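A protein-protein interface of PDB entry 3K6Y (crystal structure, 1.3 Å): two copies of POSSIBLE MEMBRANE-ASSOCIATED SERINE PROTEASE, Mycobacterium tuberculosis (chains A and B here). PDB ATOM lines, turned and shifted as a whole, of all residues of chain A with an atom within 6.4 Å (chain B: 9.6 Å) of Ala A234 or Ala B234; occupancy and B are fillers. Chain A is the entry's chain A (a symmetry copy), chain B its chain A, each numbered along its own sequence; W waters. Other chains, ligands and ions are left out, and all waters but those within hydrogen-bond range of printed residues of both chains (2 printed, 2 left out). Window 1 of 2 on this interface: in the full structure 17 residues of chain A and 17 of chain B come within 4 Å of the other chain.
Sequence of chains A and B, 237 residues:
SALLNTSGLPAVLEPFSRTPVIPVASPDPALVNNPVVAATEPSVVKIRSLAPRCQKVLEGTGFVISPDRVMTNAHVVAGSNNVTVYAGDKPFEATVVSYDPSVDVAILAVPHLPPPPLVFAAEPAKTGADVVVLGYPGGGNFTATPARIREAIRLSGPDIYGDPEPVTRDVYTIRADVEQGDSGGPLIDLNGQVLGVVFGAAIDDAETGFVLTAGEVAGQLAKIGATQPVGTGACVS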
ATOM      1  N   ARG A  53       2.973   1.140   5.730  1.00  0.00           N
ATOM      2  CA  ARG A  53       1.702   0.607   6.199  1.00  0.00           C
ATOM      3  C   ARG A  53       1.918  -0.251   7.446  1.00  0.00           C
ATOM      4  O   ARG A  53       1.023  -0.402   8.284  1.00  0.00           O
ATOM      5  CB  ARG A  53       1.062  -0.241   5.106  1.00  0.00           C
ATOM      6  CG  ARG A  53       0.062   0.441   4.220  1.00  0.00           C
ATOM      7  CD  ARG A  53      -0.846  -0.604   3.563  1.00  0.00           C
ATOM      8  NE  ARG A  53      -0.159  -1.364   2.515  1.00  0.00           N
ATOM      9  CZ  ARG A  53      -0.284  -2.679   2.325  1.00  0.00           C
ATOM     10  NH1 ARG A  53       0.356  -3.245   1.319  1.00  0.00           N
ATOM     11  NH2 ARG A  53      -1.026  -3.438   3.132  1.00  0.00           N
ATOM     12  N   CYS A  54       3.121  -0.819   7.560  1.00  0.00           N
ATOM     13  CA  CYS A  54       3.451  -1.739   8.621  1.00  0.00           C
ATOM     14  C   CYS A  54       4.316  -1.062   9.678  1.00  0.00           C
ATOM     15  O   CYS A  54       4.740  -1.709  10.625  1.00  0.00           O
ATOM     16  CB  CYS A  54       4.240  -2.939   8.043  1.00  0.00           C
ATOM     17  SG  CYS A  54       3.542  -3.643   6.537  1.00  0.00           S
ATOM     18  N   ALA A  78       6.195  -8.232   1.954  1.00  0.00           N
ATOM     19  CA  ALA A  78       4.776  -8.127   2.322  1.00  0.00           C
ATOM     20  C   ALA A  78       4.452  -6.790   2.964  1.00  0.00           C
ATOM     21  O   ALA A  78       5.117  -6.377   3.901  1.00  0.00           O
ATOM     22  CB  ALA A  78       4.414  -9.243   3.267  1.00  0.00           C
ATOM     23  N   GLY A  79       3.429  -6.120   2.442  1.00  0.00           N
ATOM     24  CA  GLY A  79       2.976  -4.855   2.999  1.00  0.00           C
ATOM     25  C   GLY A  79       3.770  -3.647   2.570  1.00  0.00           C
ATOM     26  O   GLY A  79       3.428  -2.540   2.948  1.00  0.00           O
ATOM     27  N   SER A  80       4.831  -3.848   1.788  1.00  0.00           N
ATOM     28  CA  SER A  80       5.700  -2.754   1.414  1.00  0.00           C
ATOM     29  C   SER A  80       5.159  -1.954   0.251  1.00  0.00           C
ATOM     30  O   SER A  80       4.297  -2.420  -0.498  1.00  0.00           O
ATOM     31  CB  SER A  80       7.075  -3.284   1.023  1.00  0.00           C
ATOM     32  OG  SER A  80       7.062  -4.014  -0.195  1.00  0.00           O
ATOM     33  N   TYR A  99       3.838 -12.573  -6.697  1.00  0.00           N
ATOM     34  CA  TYR A  99       3.741 -12.531  -5.252  1.00  0.00           C
ATOM     35  C   TYR A  99       2.770 -13.625  -4.845  1.00  0.00           C
ATOM     36  O   TYR A  99       1.590 -13.585  -5.217  1.00  0.00           O
ATOM     37  CB  TYR A  99       3.274 -11.143  -4.791  1.00  0.00           C
ATOM     38  CG  TYR A  99       3.146 -11.005  -3.290  1.00  0.00           C
ATOM     39  CD1 TYR A  99       4.224 -10.608  -2.501  1.00  0.00           C
ATOM     40  CD2 TYR A  99       1.931 -11.254  -2.664  1.00  0.00           C
ATOM     41  CE1 TYR A  99       4.086 -10.478  -1.126  1.00  0.00           C
ATOM     42  CE2 TYR A  99       1.796 -11.135  -1.293  1.00  0.00           C
ATOM     43  CZ  TYR A  99       2.875 -10.758  -0.540  1.00  0.00           C
ATOM     44  OH  TYR A  99       2.731 -10.643   0.817  1.00  0.00           O
ATOM     45  N   ILE A 160       1.511 -16.890   5.303  1.00  0.00           N
ATOM     46  CA  ILE A 160       2.196 -15.813   6.014  1.00  0.00           C
ATOM     47  C   ILE A 160       1.241 -14.847   6.716  1.00  0.00           C
ATOM     48  O   ILE A 160       1.655 -14.115   7.621  1.00  0.00           O
ATOM     49  CB  ILE A 160       3.182 -15.040   5.121  1.00  0.00           C
ATOM     50  CG1 ILE A 160       2.465 -14.309   3.998  1.00  0.00           C
ATOM     51  CG2 ILE A 160       4.270 -15.981   4.594  1.00  0.00           C
ATOM     52  CD1 ILE A 160       3.393 -13.385   3.211  1.00  0.00           C
ATOM     53  N   TYR A 161      -0.022 -14.836   6.293  1.00  0.00           N
ATOM     54  CA  TYR A 161      -1.018 -13.962   6.909  1.00  0.00           C
ATOM     55  C   TYR A 161      -1.816 -14.627   8.019  1.00  0.00           C
ATOM     56  O   TYR A 161      -2.653 -13.972   8.654  1.00  0.00           O
ATOM     57  CB  TYR A 161      -2.022 -13.509   5.865  1.00  0.00           C
ATOM     58  CG  TYR A 161      -1.467 -12.825   4.636  1.00  0.00           C
ATOM     59  CD1 TYR A 161      -1.957 -13.182   3.374  1.00  0.00           C
ATOM     60  CD2 TYR A 161      -0.533 -11.804   4.729  1.00  0.00           C
ATOM     61  CE1 TYR A 161      -1.535 -12.552   2.210  1.00  0.00           C
ATOM     62  CE2 TYR A 161      -0.050 -11.171   3.538  1.00  0.00           C
ATOM     63  CZ  TYR A 161      -0.575 -11.556   2.296  1.00  0.00           C
ATOM     64  OH  TYR A 161      -0.126 -10.915   1.153  1.00  0.00           O
ATOM     65  N   ASP A 163      -4.027 -16.843   7.290  1.00  0.00           N
ATOM     66  CA  ASP A 163      -5.341 -17.090   6.690  1.00  0.00           C
ATOM     67  C   ASP A 163      -5.951 -18.395   7.201  1.00  0.00           C
ATOM     68  O   ASP A 163      -5.232 -19.314   7.596  1.00  0.00           O
ATOM     69  CB  ASP A 163      -5.238 -17.162   5.154  1.00  0.00           C
ATOM     70  CG  ASP A 163      -4.917 -15.820   4.491  1.00  0.00           C
ATOM     71  OD1 ASP A 163      -5.396 -14.766   4.959  1.00  0.00           O
ATOM     72  OD2 ASP A 163      -4.178 -15.863   3.471  1.00  0.00           O
ATOM     73  N   THR A 232       1.509  -6.197  -2.776  1.00  0.00           N
ATOM     74  CA  THR A 232       2.275  -6.909  -1.759  1.00  0.00           C
ATOM     75  C   THR A 232       1.433  -7.275  -0.549  1.00  0.00           C
ATOM     76  O   THR A 232       1.973  -7.626   0.505  1.00  0.00           O
ATOM     77  CB  THR A 232       3.479  -6.108  -1.317  1.00  0.00           C
ATOM     78  OG1 THR A 232       3.011  -4.812  -0.951  1.00  0.00           O
ATOM     79  CG2 THR A 232       4.523  -6.036  -2.431  1.00  0.00           C
ATOM     80  N   GLY A 233       0.112  -7.248  -0.681  1.00  0.00           N
ATOM     81  CA  GLY A 233      -0.752  -7.806   0.349  1.00  0.00           C
ATOM     82  C   GLY A 233      -0.717  -7.081   1.686  1.00  0.00           C
ATOM     83  O   GLY A 233      -0.459  -5.875   1.782  1.00  0.00           O
ATOM     84  N   ALA A 234      -0.999  -7.831   2.744  1.00  0.00           N
ATOM     85  CA  ALA A 234      -1.101  -7.288   4.085  1.00  0.00           C
ATOM     86  C   ALA A 234       0.247  -7.311   4.774  1.00  0.00           C
ATOM     87  O   ALA A 234       1.156  -8.068   4.412  1.00  0.00           O
ATOM     88  CB  ALA A 234      -2.101  -8.094   4.895  1.00  0.00           C
ATOM     89  N   CYS A 235       0.365  -6.509   5.820  1.00  0.00           N
ATOM     90  CA  CYS A 235       1.505  -6.603   6.720  1.00  0.00           C
ATOM     91  C   CYS A 235       1.454  -7.913   7.466  1.00  0.00           C
ATOM     92  O   CYS A 235       0.381  -8.349   7.929  1.00  0.00           O
ATOM     93  CB  CYS A 235       1.479  -5.459   7.732  1.00  0.00           C
ATOM     94  SG  CYS A 235       1.540  -3.851   6.910  1.00  0.00           S
ATOM     95  N   VAL A 236       2.597  -8.568   7.581  1.00  0.00           N
ATOM     96  CA  VAL A 236       2.633  -9.787   8.370  1.00  0.00           C
ATOM     97  C   VAL A 236       2.459  -9.382   9.844  1.00  0.00           C
ATOM     98  O   VAL A 236       3.049  -8.394  10.272  1.00  0.00           O
ATOM     99  CB  VAL A 236       3.903 -10.595   8.061  1.00  0.00           C
ATOM    100  CG1 VAL A 236       4.056 -11.781   8.990  1.00  0.00           C
ATOM    101  CG2 VAL A 236       3.900 -11.074   6.616  1.00  0.00           C
ATOM    102  N   ALA B  51     -13.265 -17.639  -2.241  1.00  0.00           N
ATOM    103  CA  ALA B  51     -12.110 -17.360  -1.404  1.00  0.00           C
ATOM    104  C   ALA B  51     -11.762 -18.590  -0.558  1.00  0.00           C
ATOM    105  O   ALA B  51     -11.880 -18.567   0.675  1.00  0.00           O
ATOM    106  CB  ALA B  51     -12.351 -16.132  -0.534  1.00  0.00           C
ATOM    107  N   ARG B  53      -8.933 -19.583   0.375  1.00  0.00           N
ATOM    108  CA  ARG B  53      -7.920 -19.281   1.376  1.00  0.00           C
ATOM    109  C   ARG B  53      -8.584 -18.825   2.676  1.00  0.00           C
ATOM    110  O   ARG B  53      -8.027 -18.978   3.769  1.00  0.00           O
ATOM    111  CB  ARG B  53      -6.999 -18.180   0.864  1.00  0.00           C
ATOM    112  CG  ARG B  53      -5.727 -18.618   0.201  1.00  0.00           C
ATOM    113  CD  ARG B  53      -4.708 -17.473   0.227  1.00  0.00           C
ATOM    114  NE  ARG B  53      -5.047 -16.400  -0.712  1.00  0.00           N
ATOM    115  CZ  ARG B  53      -4.935 -15.097  -0.448  1.00  0.00           C
ATOM    116  NH1 ARG B  53      -5.232 -14.223  -1.392  1.00  0.00           N
ATOM    117  NH2 ARG B  53      -4.544 -14.654   0.747  1.00  0.00           N
ATOM    118  N   CYS B  54      -9.784 -18.255   2.548  1.00  0.00           N
ATOM    119  CA  CYS B  54     -10.496 -17.677   3.662  1.00  0.00           C
ATOM    120  C   CYS B  54     -11.626 -18.592   4.118  1.00  0.00           C
ATOM    121  O   CYS B  54     -12.373 -18.236   5.019  1.00  0.00           O
ATOM    122  CB  CYS B  54     -11.109 -16.320   3.242  1.00  0.00           C
ATOM    123  SG  CYS B  54      -9.988 -15.236   2.336  1.00  0.00           S
ATOM    124  N   LYS B  56     -14.379 -19.160   2.557  1.00  0.00           N
ATOM    125  CA  LYS B  56     -15.587 -18.350   2.366  1.00  0.00           C
ATOM    126  C   LYS B  56     -15.876 -18.163   0.884  1.00  0.00           C
ATOM    127  O   LYS B  56     -14.975 -18.233   0.045  1.00  0.00           O
ATOM    128  CB  LYS B  56     -15.401 -16.919   2.916  1.00  0.00           C
ATOM    129  CG  LYS B  56     -15.370 -16.696   4.405  1.00  0.00           C
ATOM    130  CD  LYS B  56     -15.026 -15.200   4.641  1.00  0.00           C
ATOM    131  CE  LYS B  56     -15.016 -14.867   6.126  1.00  0.00           C
ATOM    132  NZ  LYS B  56     -14.897 -13.398   6.366  1.00  0.00           N
ATOM    133  N   LEU B  58     -17.442 -14.809  -0.845  1.00  0.00           N
ATOM    134  CA  LEU B  58     -17.766 -13.410  -0.561  1.00  0.00           C
ATOM    135  C   LEU B  58     -18.757 -12.913  -1.589  1.00  0.00           C
ATOM    136  O   LEU B  58     -18.594 -13.179  -2.772  1.00  0.00           O
ATOM    137  CB  LEU B  58     -16.505 -12.552  -0.689  1.00  0.00           C
ATOM    138  CG  LEU B  58     -15.548 -12.630   0.490  1.00  0.00           C
ATOM    139  CD1 LEU B  58     -14.192 -12.034   0.094  1.00  0.00           C
ATOM    140  CD2 LEU B  58     -16.147 -11.851   1.641  1.00  0.00           C
ATOM    141  N   ALA B  74     -12.359  -3.097  -1.994  1.00  0.00           N
ATOM    142  CA  ALA B  74     -11.330  -4.123  -1.922  1.00  0.00           C
ATOM    143  C   ALA B  74     -11.802  -5.298  -1.064  1.00  0.00           C
ATOM    144  O   ALA B  74     -11.546  -6.448  -1.397  1.00  0.00           O
ATOM    145  CB  ALA B  74     -10.032  -3.548  -1.389  1.00  0.00           C
ATOM    146  N   HIS B  75     -12.511  -5.021   0.031  1.00  0.00           N
ATOM    147  CA  HIS B  75     -12.894  -6.113   0.927  1.00  0.00           C
ATOM    148  C   HIS B  75     -13.942  -7.038   0.327  1.00  0.00           C
ATOM    149  O   HIS B  75     -14.172  -8.122   0.847  1.00  0.00           O
ATOM    150  CB  HIS B  75     -13.334  -5.599   2.301  1.00  0.00           C
ATOM    151  CG  HIS B  75     -14.683  -4.934   2.317  1.00  0.00           C
ATOM    152  ND1 HIS B  75     -14.845  -3.562   2.391  1.00  0.00           N
ATOM    153  CD2 HIS B  75     -15.937  -5.457   2.338  1.00  0.00           C
ATOM    154  CE1 HIS B  75     -16.138  -3.276   2.459  1.00  0.00           C
ATOM    155  NE2 HIS B  75     -16.820  -4.407   2.416  1.00  0.00           N
ATOM    156  N   VAL B  76     -14.554  -6.653  -0.790  1.00  0.00           N
ATOM    157  CA  VAL B  76     -15.479  -7.556  -1.471  1.00  0.00           C
ATOM    158  C   VAL B  76     -14.737  -8.678  -2.208  1.00  0.00           C
ATOM    159  O   VAL B  76     -15.318  -9.732  -2.447  1.00  0.00           O
ATOM    160  CB  VAL B  76     -16.409  -6.739  -2.394  1.00  0.00           C
ATOM    161  CG1 VAL B  76     -17.209  -7.581  -3.365  1.00  0.00           C
ATOM    162  CG2 VAL B  76     -17.330  -5.912  -1.544  1.00  0.00           C
ATOM    163  N   VAL B  77     -13.453  -8.461  -2.534  1.00  0.00           N
ATOM    164  CA  VAL B  77     -12.667  -9.461  -3.239  1.00  0.00           C
ATOM    165  C   VAL B  77     -11.425  -9.911  -2.467  1.00  0.00           C
ATOM    166  O   VAL B  77     -10.695 -10.778  -2.947  1.00  0.00           O
ATOM    167  CB  VAL B  77     -12.249  -8.956  -4.677  1.00  0.00           C
ATOM    168  CG1 VAL B  77     -13.483  -8.658  -5.517  1.00  0.00           C
ATOM    169  CG2 VAL B  77     -11.329  -7.729  -4.607  1.00  0.00           C
ATOM    170  N   ALA B  78     -11.203  -9.355  -1.276  1.00  0.00           N
ATOM    171  CA  ALA B  78      -9.984  -9.639  -0.507  1.00  0.00           C
ATOM    172  C   ALA B  78      -9.822 -11.122  -0.224  1.00  0.00           C
ATOM    173  O   ALA B  78     -10.738 -11.760   0.271  1.00  0.00           O
ATOM    174  CB  ALA B  78     -10.015  -8.878   0.793  1.00  0.00           C
ATOM    175  N   GLY B  79      -8.650 -11.659  -0.550  1.00  0.00           N
ATOM    176  CA  GLY B  79      -8.342 -13.053  -0.279  1.00  0.00           C
ATOM    177  C   GLY B  79      -8.885 -14.035  -1.287  1.00  0.00           C
ATOM    178  O   GLY B  79      -8.630 -15.221  -1.166  1.00  0.00           O
ATOM    179  N   SER B  80      -9.635 -13.555  -2.280  1.00  0.00           N
ATOM    180  CA  SER B  80     -10.271 -14.440  -3.230  1.00  0.00           C
ATOM    181  C   SER B  80      -9.333 -14.883  -4.329  1.00  0.00           C
ATOM    182  O   SER B  80      -8.296 -14.261  -4.574  1.00  0.00           O
ATOM    183  CB  SER B  80     -11.464 -13.747  -3.879  1.00  0.00           C
ATOM    184  OG  SER B  80     -11.084 -12.688  -4.746  1.00  0.00           O
ATOM    185  N   TYR B  99      -6.336  -2.759  -6.936  1.00  0.00           N
ATOM    186  CA  TYR B  99      -6.723  -3.235  -5.623  1.00  0.00           C
ATOM    187  C   TYR B  99      -6.001  -2.366  -4.608  1.00  0.00           C
ATOM    188  O   TYR B  99      -4.764  -2.354  -4.562  1.00  0.00           O
ATOM    189  CB  TYR B  99      -6.363  -4.720  -5.469  1.00  0.00           C
ATOM    190  CG  TYR B  99      -6.734  -5.307  -4.126  1.00  0.00           C
ATOM    191  CD1 TYR B  99      -7.991  -5.864  -3.896  1.00  0.00           C
ATOM    192  CD2 TYR B  99      -5.811  -5.320  -3.087  1.00  0.00           C
ATOM    193  CE1 TYR B  99      -8.311  -6.405  -2.660  1.00  0.00           C
ATOM    194  CE2 TYR B  99      -6.133  -5.850  -1.852  1.00  0.00           C
ATOM    195  CZ  TYR B  99      -7.380  -6.378  -1.649  1.00  0.00           C
ATOM    196  OH  TYR B  99      -7.689  -6.900  -0.421  1.00  0.00           O
ATOM    197  N   PRO B 101      -6.207  -1.633  -0.545  1.00  0.00           N
ATOM    198  CA  PRO B 101      -6.806  -1.979   0.736  1.00  0.00           C
ATOM    199  C   PRO B 101      -6.791  -0.835   1.736  1.00  0.00           C
ATOM    200  O   PRO B 101      -7.361  -0.985   2.822  1.00  0.00           O
ATOM    201  CB  PRO B 101      -5.909  -3.119   1.213  1.00  0.00           C
ATOM    202  CG  PRO B 101      -4.574  -2.785   0.671  1.00  0.00           C
ATOM    203  CD  PRO B 101      -4.849  -2.193  -0.700  1.00  0.00           C
ATOM    204  N   SER B 102      -6.139   0.270   1.392  1.00  0.00           N
ATOM    205  CA  SER B 102      -6.088   1.448   2.262  1.00  0.00           C
ATOM    206  C   SER B 102      -7.324   2.284   2.014  1.00  0.00           C
ATOM    207  O   SER B 102      -8.076   2.595   2.942  1.00  0.00           O
ATOM    208  CB  SER B 102      -4.820   2.267   2.014  1.00  0.00           C
ATOM    209  OG  SER B 102      -3.649   1.502   2.280  1.00  0.00           O
ATOM    210  N   ASP B 159      -6.988   0.136   8.180  1.00  0.00           N
ATOM    211  CA  ASP B 159      -7.332  -0.364   6.848  1.00  0.00           C
ATOM    212  C   ASP B 159      -7.992  -1.726   6.981  1.00  0.00           C
ATOM    213  O   ASP B 159      -8.190  -2.212   8.107  1.00  0.00           O
ATOM    214  CB  ASP B 159      -6.118  -0.347   5.912  1.00  0.00           C
ATOM    215  CG  ASP B 159      -5.056  -1.394   6.239  1.00  0.00           C
ATOM    216  OD1 ASP B 159      -5.301  -2.364   6.998  1.00  0.00           O
ATOM    217  OD2 ASP B 159      -3.943  -1.221   5.683  1.00  0.00           O
ATOM    218  N   ILE B 160      -8.359  -2.350   5.863  1.00  0.00           N
ATOM    219  CA  ILE B 160      -9.185  -3.553   5.949  1.00  0.00           C
ATOM    220  C   ILE B 160      -8.467  -4.733   6.607  1.00  0.00           C
ATOM    221  O   ILE B 160      -9.120  -5.679   7.061  1.00  0.00           O
ATOM    222  CB  ILE B 160      -9.776  -3.971   4.592  1.00  0.00           C
ATOM    223  CG1 ILE B 160      -8.688  -4.370   3.607  1.00  0.00           C
ATOM    224  CG2 ILE B 160     -10.674  -2.860   4.040  1.00  0.00           C
ATOM    225  CD1 ILE B 160      -9.253  -4.967   2.319  1.00  0.00           C
ATOM    226  N   TYR B 161      -7.138  -4.684   6.644  1.00  0.00           N
ATOM    227  CA  TYR B 161      -6.359  -5.752   7.266  1.00  0.00           C
ATOM    228  C   TYR B 161      -6.010  -5.492   8.722  1.00  0.00           C
ATOM    229  O   TYR B 161      -5.399  -6.349   9.373  1.00  0.00           O
ATOM    230  CB  TYR B 161      -5.041  -5.924   6.530  1.00  0.00           C
ATOM    231  CG  TYR B 161      -5.120  -6.181   5.042  1.00  0.00           C
ATOM    232  CD1 TYR B 161      -4.258  -5.489   4.183  1.00  0.00           C
ATOM    233  CD2 TYR B 161      -5.978  -7.132   4.510  1.00  0.00           C
ATOM    234  CE1 TYR B 161      -4.236  -5.720   2.813  1.00  0.00           C
ATOM    235  CE2 TYR B 161      -6.003  -7.354   3.095  1.00  0.00           C
ATOM    236  CZ  TYR B 161      -5.116  -6.644   2.274  1.00  0.00           C
ATOM    237  OH  TYR B 161      -5.125  -6.891   0.910  1.00  0.00           O
ATOM    238  N   GLY B 162      -6.335  -4.307   9.222  1.00  0.00           N
ATOM    239  CA  GLY B 162      -5.879  -3.942  10.561  1.00  0.00           C
ATOM    240  C   GLY B 162      -4.373  -3.752  10.578  1.00  0.00           C
ATOM    241  O   GLY B 162      -3.725  -4.016  11.593  1.00  0.00           O
ATOM    242  N   ASP B 163      -3.803  -3.279   9.467  1.00  0.00           N
ATOM    243  CA  ASP B 163      -2.379  -2.932   9.441  1.00  0.00           C
ATOM    244  C   ASP B 163      -2.043  -1.874  10.491  1.00  0.00           C
ATOM    245  O   ASP B 163      -2.899  -1.078  10.879  1.00  0.00           O
ATOM    246  CB  ASP B 163      -1.968  -2.400   8.055  1.00  0.00           C
ATOM    247  CG  ASP B 163      -1.980  -3.464   6.954  1.00  0.00           C
ATOM    248  OD1 ASP B 163      -1.629  -4.633   7.217  1.00  0.00           O
ATOM    249  OD2 ASP B 163      -2.340  -3.080   5.808  1.00  0.00           O
ATOM    250  N   PRO B 164      -0.779  -1.850  10.944  1.00  0.00           N
ATOM    251  CA  PRO B 164      -0.341  -0.858  11.941  1.00  0.00           C
ATOM    252  C   PRO B 164      -0.690   0.616  11.674  1.00  0.00           C
ATOM    253  O   PRO B 164      -1.177   1.302  12.581  1.00  0.00           O
ATOM    254  CB  PRO B 164       1.188  -1.071  11.975  1.00  0.00           C
ATOM    255  CG  PRO B 164       1.326  -2.531  11.729  1.00  0.00           C
ATOM    256  CD  PRO B 164       0.291  -2.829  10.655  1.00  0.00           C
ATOM    257  N   GLY B 231      -2.721  -8.912  -7.105  1.00  0.00           N
ATOM    258  CA  GLY B 231      -3.283  -9.850  -6.114  1.00  0.00           C
ATOM    259  C   GLY B 231      -4.479  -9.279  -5.358  1.00  0.00           C
ATOM    260  O   GLY B 231      -4.779  -8.075  -5.439  1.00  0.00           O
ATOM    261  N   THR B 232      -5.112 -10.128  -4.557  1.00  0.00           N
ATOM    262  CA  THR B 232      -6.208  -9.713  -3.690  1.00  0.00           C
ATOM    263  C   THR B 232      -5.837  -9.770  -2.217  1.00  0.00           C
ATOM    264  O   THR B 232      -6.714  -9.721  -1.349  1.00  0.00           O
ATOM    265  CB  THR B 232      -7.448 -10.544  -3.933  1.00  0.00           C
ATOM    266  OG1 THR B 232      -7.061 -11.914  -3.837  1.00  0.00           O
ATOM    267  CG2 THR B 232      -8.056 -10.226  -5.299  1.00  0.00           C
ATOM    268  N   GLY B 233      -4.548  -9.825  -1.904  1.00  0.00           N
ATOM    269  CA  GLY B 233      -4.106  -9.645  -0.529  1.00  0.00           C
ATOM    270  C   GLY B 233      -4.545 -10.734   0.439  1.00  0.00           C
ATOM    271  O   GLY B 233      -4.757 -11.898   0.079  1.00  0.00           O
ATOM    272  N   ALA B 234      -4.671 -10.349   1.703  1.00  0.00           N
ATOM    273  CA  ALA B 234      -4.992 -11.274   2.774  1.00  0.00           C
ATOM    274  C   ALA B 234      -6.492 -11.387   2.948  1.00  0.00           C
ATOM    275  O   ALA B 234      -7.267 -10.510   2.550  1.00  0.00           O
ATOM    276  CB  ALA B 234      -4.362 -10.799   4.072  1.00  0.00           C
ATOM    277  N   CYS B 235      -6.908 -12.456   3.606  1.00  0.00           N
ATOM    278  CA  CYS B 235      -8.286 -12.577   4.060  1.00  0.00           C
ATOM    279  C   CYS B 235      -8.554 -11.552   5.136  1.00  0.00           C
ATOM    280  O   CYS B 235      -7.721 -11.332   6.037  1.00  0.00           O
ATOM    281  CB  CYS B 235      -8.538 -13.970   4.633  1.00  0.00           C
ATOM    282  SG  CYS B 235      -8.238 -15.255   3.398  1.00  0.00           S
ATOM    283  N   VAL B 236      -9.703 -10.904   5.054  1.00  0.00           N
ATOM    284  CA  VAL B 236     -10.064  -9.976   6.113  1.00  0.00           C
ATOM    285  C   VAL B 236     -10.368 -10.811   7.369  1.00  0.00           C
ATOM    286  O   VAL B 236     -11.015 -11.849   7.259  1.00  0.00           O
ATOM    287  CB  VAL B 236     -11.199  -9.047   5.655  1.00  0.00           C
ATOM    288  CG1 VAL B 236     -11.714  -8.186   6.789  1.00  0.00           C
ATOM    289  CG2 VAL B 236     -10.741  -8.159   4.507  1.00  0.00           C
ATOM    290  N   SER B 237      -9.853 -10.388   8.526  1.00  0.00           N
ATOM    291  CA  SER B 237     -10.025 -11.157   9.773  1.00  0.00           C
ATOM    292  C   SER B 237     -11.475 -11.165  10.236  1.00  0.00           C
ATOM    293  O   SER B 237     -12.285 -10.295   9.885  1.00  0.00           O
ATOM    294  CB  SER B 237      -9.125 -10.617  10.893  1.00  0.00           C
ATOM    295  OG  SER B 237      -7.764 -10.627  10.510  1.00  0.00           O
ATOM    296  OXT SER B 237     -11.863 -12.070  10.978  1.00  0.00           O
HETATM  297  O   HOH W   1      -3.105  -5.875  -0.450  1.00  0.00           O
HETATM  298  O   HOH W   2      -1.523 -11.371  -1.039  1.00  0.00           O
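The side-chain carboxylate (OD2) of Asp A163 is in salt-bridge range of the guanidinium group (NH2) of Arg B53.
OD2 of Asp B163 is in salt-bridge range of NH2 of Arg A53 (3.0 Å).
The side-chain carboxylate (OD1) of Asp B163 sits at hydrogen-bond distance from the backbone NH (N) of Cys A235.
The side-chain carboxylate (OD1) of Asp A163 sits at hydrogen-bond distance from the backbone NH (N) of Cys B235, 3.1 Å away.
The side-chain sulfur (SG) of Cys B235 is disulfide-bonded to the side-chain sulfur (SG) of Cys B54, at 2.0 Å.
OD1 of Asp B159 sits at hydrogen-bond distance from N of Gly B162, 3.1 Å away.
The backbone NH (N) of Asp B163 lies within hydrogen-bond range of the side-chain carboxylate (OD1) of Asp B159 (3.0 Å).
The backbone carbonyl oxygen (O) of Gly A233 lies within hydrogen-bond range of the guanidinium group (NH1) of Arg A53 (2.8 Å).
The side-chain sulfur of Cys A235 forms a disulfide with the side-chain sulfur of Cys A54 (2.0 Å).
The side-chain hydroxyl of Tyr A161 lies within hydrogen-bond range of the side-chain hydroxyl of Tyr A99, 2.9 Å away.
Among the printed residues, pairs that only touch across the chains: Arg A53 with Ser B102, Arg A53 with Asp B159, Arg A53 with Tyr B161, Arg A53 with Pro B164, Cys A54 with Pro B164, Tyr A161 with Arg B53, Tyr A161 with Gly B233, Tyr A161 with Ala B234, Gly A233 with Tyr B161, Gly A233 with Gly B233, Ala A234 with Tyr B161 and Ala A234 with Ala B234.
Of the printed residues of chain B, Arg A53 touches Ser B102 (3.7 Å), Asp B159 (3.8 Å), Tyr B161 (3.95 Å), Asp B163 (3.0 Å) and Pro B164 (3.5 Å).
Of chain B, only Tyr B161 (3.9 Å) and Gly B233 (3.9 Å) come within 4 Å of Gly A233.
Ala A234 touches just these residues of chain B: Tyr B161 and Ala B234.
Cys A235 touches one residue of chain B.
Ala B74 touches none of the printed residues of chain A.
Gly B79 touches none of the printed residues of chain A.
Printed residues of chain A within 4 Å of Asp B163: Arg A53 (3.0 Å) and Cys A235 (3.1 Å).
Ala B234 touches two residues of chain A.
The nearest residue of chain A that does not touch Ala B234 is Asp A163 (4.1 Å).
The nearest printed residue of chain A that does not touch Tyr B161 is Cys A235 (5.0 Å).
Of the 28 printed residues of chain B, 9 touch a printed residue of chain A.
Hydrophobic or aromatic side chains of chain B within 4 Å of the printed part of chain A: Tyr B161, Pro B164 and Ala B234.
Of the 14 printed residues of chain A, 7 touch a printed residue of chain B.
Along chain A the printed residues that touch a printed residue of chain B span positions 53 to 235.
Among the printed residues, Asp or Glu carboxylates within 4 Å of a Lys or Arg side-chain nitrogen of the other chain: Arg A53 with Asp B163 and Asp A163 with Arg B53.
Arg A53 touches Asp B163, and with the chains exchanged Asp A163 touches Arg B53.
Tyr A161 touches Gly B233, and with the chains exchanged Gly A233 touches Tyr B161.
Asp A163 touches Cys B235, and with the chains exchanged Cys A235 touches Asp B163.
Ala B234 touches its own counterpart, Ala A234.
Water W2 bridges the side-chain hydroxyl of Tyr A161 (2.6 Å) and the backbone carbonyl oxygen of Gly B233 (3.5 Å).
Water W1 bridges OH of Tyr B161 (2.6 Å) and O of Gly A233 (3.5 Å).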
